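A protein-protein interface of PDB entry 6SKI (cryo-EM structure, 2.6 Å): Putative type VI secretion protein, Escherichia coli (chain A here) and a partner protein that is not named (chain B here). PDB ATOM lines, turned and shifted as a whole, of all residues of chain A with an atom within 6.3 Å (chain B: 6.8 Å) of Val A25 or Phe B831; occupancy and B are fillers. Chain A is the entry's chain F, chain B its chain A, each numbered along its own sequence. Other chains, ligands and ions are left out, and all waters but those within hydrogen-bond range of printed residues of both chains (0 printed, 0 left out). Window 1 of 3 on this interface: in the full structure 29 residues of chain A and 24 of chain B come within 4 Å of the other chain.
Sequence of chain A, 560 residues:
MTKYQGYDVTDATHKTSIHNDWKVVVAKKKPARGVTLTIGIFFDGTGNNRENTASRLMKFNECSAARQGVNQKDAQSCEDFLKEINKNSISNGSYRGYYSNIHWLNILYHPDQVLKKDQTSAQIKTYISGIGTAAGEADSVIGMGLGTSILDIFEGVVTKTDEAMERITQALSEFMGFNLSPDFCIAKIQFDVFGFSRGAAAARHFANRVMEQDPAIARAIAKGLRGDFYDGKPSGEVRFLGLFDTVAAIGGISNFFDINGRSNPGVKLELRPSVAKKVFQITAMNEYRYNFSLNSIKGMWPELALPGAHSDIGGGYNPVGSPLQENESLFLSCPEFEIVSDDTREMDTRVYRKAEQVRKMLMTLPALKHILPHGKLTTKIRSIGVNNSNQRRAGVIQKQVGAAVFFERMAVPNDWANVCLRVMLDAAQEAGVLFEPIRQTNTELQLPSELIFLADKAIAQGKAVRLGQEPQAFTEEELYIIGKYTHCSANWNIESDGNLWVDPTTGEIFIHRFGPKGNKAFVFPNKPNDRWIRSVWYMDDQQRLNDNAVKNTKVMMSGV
Of the printed residues of chain B, Gly A6 touches Lys B833 (3.9 Å). Of the printed residues of chain B, Tyr A7 touches Thr B794 and Gly B832. Of chain B, only Phe B781 (3.4 Å), Ile B782 (2.3 Å), Leu B783 (3.4 Å), Thr B784 (3.2 Å) and Phe B831 (3.9 Å) come within 4 Å of Val A25. Of the printed residues of chain B, Ala A27 touches Leu B783, Thr B784 and Asp B785. Of the printed residues of chain A, Thr B794 touches Tyr A7 (3.2 Å). Printed residues of chain A within 4 Å of Val B829: Ala A12. Glu B830 touches none of the printed residues of chain A. Of chain A, only Val A25 (3.9 Å) comes within 4 Å of Phe B831. The nearest residue of chain B that does not touch Val A25 is Val B829 (4.7 Å).
CA of Gly A6 touches NZ of Lys B833, at 3.9 Å. Phe B781 touches Lys A23. Ile B782 touches Val A24 (O to C, 3.2 Å). Val A24 touches Thr B784 (CG2 to OG1, 3.2 Å). CD2 of Phe B781 touches CG2 of Val A25, 3.4 Å away. O of Val A25 touches CD1 of Leu B783, at 3.4 Å. Phe B831 touches Val A25 (CE2 to CG1, 3.9 Å). O of Thr B784 touches CA of Val A26, 3.3 Å away. O of Asp B785 touches CG2 of Val A26, at 3.3 Å. CB of Ala A27 touches CD1 of Leu B783, 3.8 Å away.
The side-chain hydroxyl of Tyr A7 sits close to the side-chain hydroxyl of Thr B794 (3.4 Å). The backbone carbonyl oxygen (O) of Ala A12 sits at hydrogen-bond distance from the backbone NH (N) of Val B829 (3.1 Å). The backbone NH of Lys A23 lies within hydrogen-bond range of the backbone carbonyl oxygen of Gly B780 (3.2 Å). N of Ile B782 is in hydrogen-bond range of O of Lys A23 (2.8 Å). The backbone carbonyl oxygen (O) of Val A25 is in hydrogen-bond range of the backbone NH (N) of Thr B784 (3.2 Å). The backbone carbonyl oxygen (O) of Thr B784 lies within hydrogen-bond range of the backbone NH (N) of Ala A27, at 2.8 Å. The backbone NH (N) of Val A25 sits close to the backbone carbonyl oxygen (O) of Ile B782 (2.3 Å). OD2 of Asp B785 sits close to O of Ala A27.
Hydrophobic or aromatic side chains of chain B within 4 Å of the printed part of chain A: Phe B781, Ile B782, Leu B783 and Phe B831. Hydrophobic or aromatic side chains of chain A that line the printed part of chain B: Tyr A7, Ala A12, Val A24, Val A25, Val A26 and Ala A27. Among the printed residues, no Asp or Glu carboxylate lies within 4 Å of a Lys or Arg side-chain nitrogen of the other chain.
The backbone NH (N) of Thr B816 is in hydrogen-bond range of the backbone carbonyl oxygen (O) of Phe B781. The backbone carbonyl oxygen (O) of Gly B814 is in hydrogen-bond range of the backbone NH (N) of Leu B783, at 2.6 Å. N of Thr B810 is in hydrogen-bond range of O of Thr B794 (2.8 Å). The backbone carbonyl oxygen (O) of Pro B795 sits at hydrogen-bond distance from the backbone NH (N) of Gly B832.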
ATOM      1  N   GLY A   6       9.099  12.826  18.389  1.00  0.00           N
ATOM      2  CA  GLY A   6      10.203  11.994  18.802  1.00  0.00           C
ATOM      3  C   GLY A   6       9.773  10.538  18.793  1.00  0.00           C
ATOM      4  O   GLY A   6       8.604  10.217  18.584  1.00  0.00           O
ATOM      5  N   TYR A   7      10.747   9.660  19.005  1.00  0.00           N
ATOM      6  CA  TYR A   7      10.513   8.224  18.950  1.00  0.00           C
ATOM      7  C   TYR A   7      10.931   7.600  20.270  1.00  0.00           C
ATOM      8  O   TYR A   7      12.113   7.632  20.627  1.00  0.00           O
ATOM      9  CB  TYR A   7      11.277   7.608  17.780  1.00  0.00           C
ATOM     10  CG  TYR A   7      10.837   8.175  16.454  1.00  0.00           C
ATOM     11  CD1 TYR A   7       9.754   7.644  15.778  1.00  0.00           C
ATOM     12  CD2 TYR A   7      11.484   9.268  15.899  1.00  0.00           C
ATOM     13  CE1 TYR A   7       9.342   8.170  14.576  1.00  0.00           C
ATOM     14  CE2 TYR A   7      11.076   9.802  14.700  1.00  0.00           C
ATOM     15  CZ  TYR A   7      10.007   9.249  14.041  1.00  0.00           C
ATOM     16  OH  TYR A   7       9.596   9.776  12.839  1.00  0.00           O
ATOM     17  N   VAL A   9      11.877   4.491  22.269  1.00  0.00           N
ATOM     18  CA  VAL A   9      12.544   3.281  21.808  1.00  0.00           C
ATOM     19  C   VAL A   9      12.532   2.262  22.938  1.00  0.00           C
ATOM     20  O   VAL A   9      13.131   2.484  23.995  1.00  0.00           O
ATOM     21  CB  VAL A   9      13.975   3.578  21.345  1.00  0.00           C
ATOM     22  CG1 VAL A   9      14.537   2.400  20.585  1.00  0.00           C
ATOM     23  CG2 VAL A   9      14.001   4.831  20.485  1.00  0.00           C
ATOM     24  N   THR A  10      11.846   1.139  22.721  1.00  0.00           N
ATOM     25  CA  THR A  10      11.875   0.057  23.700  1.00  0.00           C
ATOM     26  C   THR A  10      13.241  -0.621  23.728  1.00  0.00           C
ATOM     27  O   THR A  10      13.876  -0.714  24.784  1.00  0.00           O
ATOM     28  CB  THR A  10      10.775  -0.960  23.393  1.00  0.00           C
ATOM     29  N   ASP A  11      13.711  -1.093  22.575  1.00  0.00           N
ATOM     30  CA  ASP A  11      15.014  -1.731  22.445  1.00  0.00           C
ATOM     31  C   ASP A  11      15.865  -0.944  21.460  1.00  0.00           C
ATOM     32  O   ASP A  11      15.416  -0.632  20.353  1.00  0.00           O
ATOM     33  CB  ASP A  11      14.874  -3.181  21.975  1.00  0.00           C
ATOM     34  N   ALA A  12      17.109  -0.643  21.857  1.00  0.00           N
ATOM     35  CA  ALA A  12      17.929   0.291  21.091  1.00  0.00           C
ATOM     36  C   ALA A  12      19.368  -0.183  20.930  1.00  0.00           C
ATOM     37  O   ALA A  12      20.278   0.646  20.823  1.00  0.00           O
ATOM     38  CB  ALA A  12      17.927   1.678  21.741  1.00  0.00           C
ATOM     39  N   THR A  13      19.600  -1.493  20.906  1.00  0.00           N
ATOM     40  CA  THR A  13      20.959  -2.007  20.831  1.00  0.00           C
ATOM     41  C   THR A  13      21.023  -3.117  19.795  1.00  0.00           C
ATOM     42  O   THR A  13      20.012  -3.738  19.456  1.00  0.00           O
ATOM     43  CB  THR A  13      21.446  -2.527  22.190  1.00  0.00           C
ATOM     44  OG1 THR A  13      20.401  -3.277  22.823  1.00  0.00           O
ATOM     45  CG2 THR A  13      21.850  -1.372  23.089  1.00  0.00           C
ATOM     46  N   LYS A  23      18.816  -4.478  11.707  1.00  0.00           N
ATOM     47  CA  LYS A  23      17.813  -4.890  12.678  1.00  0.00           C
ATOM     48  C   LYS A  23      16.778  -3.794  12.845  1.00  0.00           C
ATOM     49  O   LYS A  23      17.131  -2.636  13.092  1.00  0.00           O
ATOM     50  CB  LYS A  23      18.452  -5.199  14.030  1.00  0.00           C
ATOM     51  N   VAL A  24      15.502  -4.163  12.715  1.00  0.00           N
ATOM     52  CA  VAL A  24      14.433  -3.196  12.912  1.00  0.00           C
ATOM     53  C   VAL A  24      14.472  -2.678  14.342  1.00  0.00           C
ATOM     54  O   VAL A  24      14.802  -3.407  15.288  1.00  0.00           O
ATOM     55  CB  VAL A  24      13.063  -3.809  12.568  1.00  0.00           C
ATOM     56  CG1 VAL A  24      12.484  -4.574  13.750  1.00  0.00           C
ATOM     57  CG2 VAL A  24      12.097  -2.723  12.128  1.00  0.00           C
ATOM     58  N   VAL A  25      14.187  -1.390  14.495  1.00  0.00           N
ATOM     59  CA  VAL A  25      14.076  -0.778  15.810  1.00  0.00           C
ATOM     60  C   VAL A  25      12.709  -0.123  15.897  1.00  0.00           C
ATOM     61  O   VAL A  25      12.550   1.055  15.565  1.00  0.00           O
ATOM     62  CB  VAL A  25      15.202   0.246  16.039  1.00  0.00           C
ATOM     63  CG1 VAL A  25      15.170   0.763  17.456  1.00  0.00           C
ATOM     64  CG2 VAL A  25      16.544  -0.382  15.734  1.00  0.00           C
ATOM     65  N   VAL A  26      11.712  -0.883  16.346  1.00  0.00           N
ATOM     66  CA  VAL A  26      10.368  -0.337  16.458  1.00  0.00           C
ATOM     67  C   VAL A  26      10.342   0.670  17.595  1.00  0.00           C
ATOM     68  O   VAL A  26      10.765   0.377  18.720  1.00  0.00           O
ATOM     69  CB  VAL A  26       9.343  -1.461  16.662  1.00  0.00           C
ATOM     70  CG1 VAL A  26       8.133  -0.947  17.420  1.00  0.00           C
ATOM     71  CG2 VAL A  26       8.924  -2.032  15.322  1.00  0.00           C
ATOM     72  N   ALA A  27       9.848   1.865  17.303  1.00  0.00           N
ATOM     73  CA  ALA A  27       9.757   2.927  18.289  1.00  0.00           C
ATOM     74  C   ALA A  27       8.446   3.660  18.079  1.00  0.00           C
ATOM     75  O   ALA A  27       8.077   3.960  16.941  1.00  0.00           O
ATOM     76  CB  ALA A  27      10.939   3.896  18.174  1.00  0.00           C
ATOM     77  N   GLY B 780      23.737  -2.338  11.142  1.00  0.00           N
ATOM     78  CA  GLY B 780      23.077  -1.070  11.394  1.00  0.00           C
ATOM     79  C   GLY B 780      21.665  -1.298  11.884  1.00  0.00           C
ATOM     80  O   GLY B 780      21.233  -2.433  12.110  1.00  0.00           O
ATOM     81  N   PHE B 781      20.944  -0.192  12.040  1.00  0.00           N
ATOM     82  CA  PHE B 781      19.594  -0.199  12.581  1.00  0.00           C
ATOM     83  C   PHE B 781      18.580   0.196  11.515  1.00  0.00           C
ATOM     84  O   PHE B 781      18.919   0.765  10.475  1.00  0.00           O
ATOM     85  CB  PHE B 781      19.473   0.762  13.767  1.00  0.00           C
ATOM     86  CG  PHE B 781      20.399   0.452  14.902  1.00  0.00           C
ATOM     87  CD1 PHE B 781      21.687   0.955  14.917  1.00  0.00           C
ATOM     88  CD2 PHE B 781      19.976  -0.321  15.965  1.00  0.00           C
ATOM     89  CE1 PHE B 781      22.537   0.680  15.963  1.00  0.00           C
ATOM     90  CE2 PHE B 781      20.818  -0.596  17.012  1.00  0.00           C
ATOM     91  CZ  PHE B 781      22.103  -0.097  17.011  1.00  0.00           C
ATOM     92  N   ILE B 782      17.316  -0.110  11.798  1.00  0.00           N
ATOM     93  CA  ILE B 782      16.197   0.277  10.947  1.00  0.00           C
ATOM     94  C   ILE B 782      15.072   0.768  11.845  1.00  0.00           C
ATOM     95  O   ILE B 782      14.582   0.019  12.694  1.00  0.00           O
ATOM     96  CB  ILE B 782      15.703  -0.883  10.060  1.00  0.00           C
ATOM     97  CG1 ILE B 782      16.807  -1.348   9.109  1.00  0.00           C
ATOM     98  CG2 ILE B 782      14.458  -0.470   9.285  1.00  0.00           C
ATOM     99  CD1 ILE B 782      16.341  -2.371   8.101  1.00  0.00           C
ATOM    100  N   LEU B 783      14.655   2.015  11.653  1.00  0.00           N
ATOM    101  CA  LEU B 783      13.644   2.635  12.498  1.00  0.00           C
ATOM    102  C   LEU B 783      12.266   2.443  11.885  1.00  0.00           C
ATOM    103  O   LEU B 783      12.053   2.755  10.710  1.00  0.00           O
ATOM    104  CB  LEU B 783      13.925   4.124  12.692  1.00  0.00           C
ATOM    105  CG  LEU B 783      12.971   4.834  13.653  1.00  0.00           C
ATOM    106  CD1 LEU B 783      13.173   4.359  15.081  1.00  0.00           C
ATOM    107  CD2 LEU B 783      13.149   6.330  13.561  1.00  0.00           C
ATOM    108  N   THR B 784      11.337   1.930  12.684  1.00  0.00           N
ATOM    109  CA  THR B 784       9.967   1.714  12.250  1.00  0.00           C
ATOM    110  C   THR B 784       9.045   2.103  13.399  1.00  0.00           C
ATOM    111  O   THR B 784       9.475   2.225  14.549  1.00  0.00           O
ATOM    112  CB  THR B 784       9.758   0.254  11.820  1.00  0.00           C
ATOM    113  OG1 THR B 784      10.794  -0.120  10.906  1.00  0.00           O
ATOM    114  CG2 THR B 784       8.426   0.067  11.124  1.00  0.00           C
ATOM    115  N   ASP B 785       7.770   2.312  13.086  1.00  0.00           N
ATOM    116  CA  ASP B 785       6.790   2.580  14.124  1.00  0.00           C
ATOM    117  C   ASP B 785       6.316   1.272  14.758  1.00  0.00           C
ATOM    118  O   ASP B 785       6.656   0.172  14.313  1.00  0.00           O
ATOM    119  CB  ASP B 785       5.608   3.364  13.556  1.00  0.00           C
ATOM    120  CG  ASP B 785       4.840   4.114  14.624  1.00  0.00           C
ATOM    121  OD1 ASP B 785       3.593   4.036  14.632  1.00  0.00           O
ATOM    122  OD2 ASP B 785       5.482   4.774  15.464  1.00  0.00           O
ATOM    123  N   THR B 794      14.487  10.508  10.142  1.00  0.00           N
ATOM    124  CA  THR B 794      14.787  10.704  11.551  1.00  0.00           C
ATOM    125  C   THR B 794      16.289  10.887  11.757  1.00  0.00           C
ATOM    126  O   THR B 794      17.090  10.165  11.155  1.00  0.00           O
ATOM    127  CB  THR B 794      14.292   9.513  12.367  1.00  0.00           C
ATOM    128  OG1 THR B 794      12.897   9.309  12.114  1.00  0.00           O
ATOM    129  CG2 THR B 794      14.501   9.756  13.850  1.00  0.00           C
ATOM    130  N   PRO B 795      16.705  11.844  12.580  1.00  0.00           N
ATOM    131  CA  PRO B 795      18.114  11.903  12.983  1.00  0.00           C
ATOM    132  C   PRO B 795      18.462  10.757  13.919  1.00  0.00           C
ATOM    133  O   PRO B 795      17.610  10.230  14.636  1.00  0.00           O
ATOM    134  CB  PRO B 795      18.220  13.254  13.700  1.00  0.00           C
ATOM    135  CG  PRO B 795      17.066  14.043  13.174  1.00  0.00           C
ATOM    136  CD  PRO B 795      15.971  13.040  13.016  1.00  0.00           C
ATOM    137  N   TYR B 796      19.736  10.374  13.909  1.00  0.00           N
ATOM    138  CA  TYR B 796      20.206   9.299  14.767  1.00  0.00           C
ATOM    139  C   TYR B 796      21.623   9.590  15.242  1.00  0.00           C
ATOM    140  O   TYR B 796      22.341  10.408  14.666  1.00  0.00           O
ATOM    141  CB  TYR B 796      20.142   7.933  14.060  1.00  0.00           C
ATOM    142  CG  TYR B 796      21.032   7.796  12.843  1.00  0.00           C
ATOM    143  CD1 TYR B 796      20.485   7.745  11.572  1.00  0.00           C
ATOM    144  CD2 TYR B 796      22.412   7.695  12.962  1.00  0.00           C
ATOM    145  CE1 TYR B 796      21.280   7.619  10.462  1.00  0.00           C
ATOM    146  CE2 TYR B 796      23.215   7.576  11.855  1.00  0.00           C
ATOM    147  CZ  TYR B 796      22.643   7.534  10.607  1.00  0.00           C
ATOM    148  OH  TYR B 796      23.436   7.410   9.496  1.00  0.00           O
ATOM    149  N   ARG B 797      22.007   8.902  16.313  1.00  0.00           N
ATOM    150  CA  ARG B 797      23.379   8.903  16.814  1.00  0.00           C
ATOM    151  C   ARG B 797      23.699   7.485  17.260  1.00  0.00           C
ATOM    152  O   ARG B 797      23.194   7.035  18.293  1.00  0.00           O
ATOM    153  CB  ARG B 797      23.560   9.880  17.973  1.00  0.00           C
ATOM    154  CG  ARG B 797      24.996  10.323  18.179  1.00  0.00           C
ATOM    155  CD  ARG B 797      25.063  11.675  18.852  1.00  0.00           C
ATOM    156  NE  ARG B 797      24.039  11.810  19.882  1.00  0.00           N
ATOM    157  CZ  ARG B 797      23.174  12.814  19.948  1.00  0.00           C
ATOM    158  NH1 ARG B 797      23.204  13.777  19.039  1.00  0.00           N
ATOM    159  NH2 ARG B 797      22.279  12.853  20.924  1.00  0.00           N
ATOM    160  N   THR B 810      18.397   8.859   9.006  1.00  0.00           N
ATOM    161  CA  THR B 810      17.977   7.611   8.380  1.00  0.00           C
ATOM    162  C   THR B 810      17.552   7.833   6.932  1.00  0.00           C
ATOM    163  O   THR B 810      17.214   8.944   6.520  1.00  0.00           O
ATOM    164  CB  THR B 810      16.833   6.967   9.167  1.00  0.00           C
ATOM    165  OG1 THR B 810      15.601   7.630   8.864  1.00  0.00           O
ATOM    166  CG2 THR B 810      17.104   7.032  10.655  1.00  0.00           C
ATOM    167  N   GLY B 814      14.126   4.147   6.526  1.00  0.00           N
ATOM    168  CA  GLY B 814      14.458   4.303   7.925  1.00  0.00           C
ATOM    169  C   GLY B 814      15.674   3.511   8.348  1.00  0.00           C
ATOM    170  O   GLY B 814      15.672   2.900   9.418  1.00  0.00           O
ATOM    171  N   THR B 816      19.800   3.238   9.190  1.00  0.00           N
ATOM    172  CA  THR B 816      20.985   3.941   9.643  1.00  0.00           C
ATOM    173  C   THR B 816      22.108   3.776   8.613  1.00  0.00           C
ATOM    174  O   THR B 816      22.000   3.006   7.657  1.00  0.00           O
ATOM    175  CB  THR B 816      21.385   3.405  11.020  1.00  0.00           C
ATOM    176  OG1 THR B 816      20.231   3.400  11.868  1.00  0.00           O
ATOM    177  CG2 THR B 816      22.421   4.273  11.684  1.00  0.00           C
ATOM    178  N   VAL B 829      21.827   2.974  19.391  1.00  0.00           N
ATOM    179  CA  VAL B 829      21.391   4.076  18.545  1.00  0.00           C
ATOM    180  C   VAL B 829      20.465   4.979  19.347  1.00  0.00           C
ATOM    181  O   VAL B 829      19.588   4.498  20.076  1.00  0.00           O
ATOM    182  CB  VAL B 829      20.713   3.565  17.260  1.00  0.00           C
ATOM    183  CG1 VAL B 829      19.392   2.882  17.569  1.00  0.00           C
ATOM    184  CG2 VAL B 829      20.508   4.706  16.277  1.00  0.00           C
ATOM    185  N   GLU B 830      20.697   6.283  19.254  1.00  0.00           N
ATOM    186  CA  GLU B 830      19.809   7.293  19.808  1.00  0.00           C
ATOM    187  C   GLU B 830      19.174   8.051  18.654  1.00  0.00           C
ATOM    188  O   GLU B 830      19.884   8.585  17.798  1.00  0.00           O
ATOM    189  CB  GLU B 830      20.572   8.254  20.722  1.00  0.00           C
ATOM    190  CG  GLU B 830      21.099   7.615  21.994  1.00  0.00           C
ATOM    191  CD  GLU B 830      22.601   7.408  21.967  1.00  0.00           C
ATOM    192  OE1 GLU B 830      23.046   6.246  22.072  1.00  0.00           O
ATOM    193  OE2 GLU B 830      23.338   8.408  21.845  1.00  0.00           O
ATOM    194  N   PHE B 831      17.846   8.094  18.627  1.00  0.00           N
ATOM    195  CA  PHE B 831      17.111   8.727  17.541  1.00  0.00           C
ATOM    196  C   PHE B 831      16.633  10.108  17.967  1.00  0.00           C
ATOM    197  O   PHE B 831      16.089  10.272  19.063  1.00  0.00           O
ATOM    198  CB  PHE B 831      15.926   7.864  17.111  1.00  0.00           C
ATOM    199  CG  PHE B 831      16.326   6.607  16.399  1.00  0.00           C
ATOM    200  CD1 PHE B 831      16.943   6.663  15.163  1.00  0.00           C
ATOM    201  CD2 PHE B 831      16.090   5.370  16.967  1.00  0.00           C
ATOM    202  CE1 PHE B 831      17.313   5.510  14.508  1.00  0.00           C
ATOM    203  CE2 PHE B 831      16.457   4.215  16.315  1.00  0.00           C
ATOM    204  CZ  PHE B 831      17.070   4.284  15.086  1.00  0.00           C
ATOM    205  N   GLY B 832      16.826  11.089  17.097  1.00  0.00           N
ATOM    206  CA  GLY B 832      16.471  12.465  17.376  1.00  0.00           C
ATOM    207  C   GLY B 832      15.009  12.756  17.126  1.00  0.00           C
ATOM    208  O   GLY B 832      14.145  11.885  17.257  1.00  0.00           O
ATOM    209  N   LYS B 833      14.728  14.001  16.757  1.00  0.00           N
ATOM    210  CA  LYS B 833      13.366  14.469  16.564  1.00  0.00           C
ATOM    211  C   LYS B 833      13.173  14.933  15.127  1.00  0.00           C
ATOM    212  O   LYS B 833      14.130  15.269  14.426  1.00  0.00           O
ATOM    213  CB  LYS B 833      13.029  15.608  17.531  1.00  0.00           C
ATOM    214  CG  LYS B 833      13.659  15.458  18.901  1.00  0.00           C
ATOM    215  CD  LYS B 833      12.693  14.868  19.906  1.00  0.00           C
ATOM    216  CE  LYS B 833      13.439  14.163  21.019  1.00  0.00           C
ATOM    217  NZ  LYS B 833      12.604  13.119  21.666  1.00  0.00           N
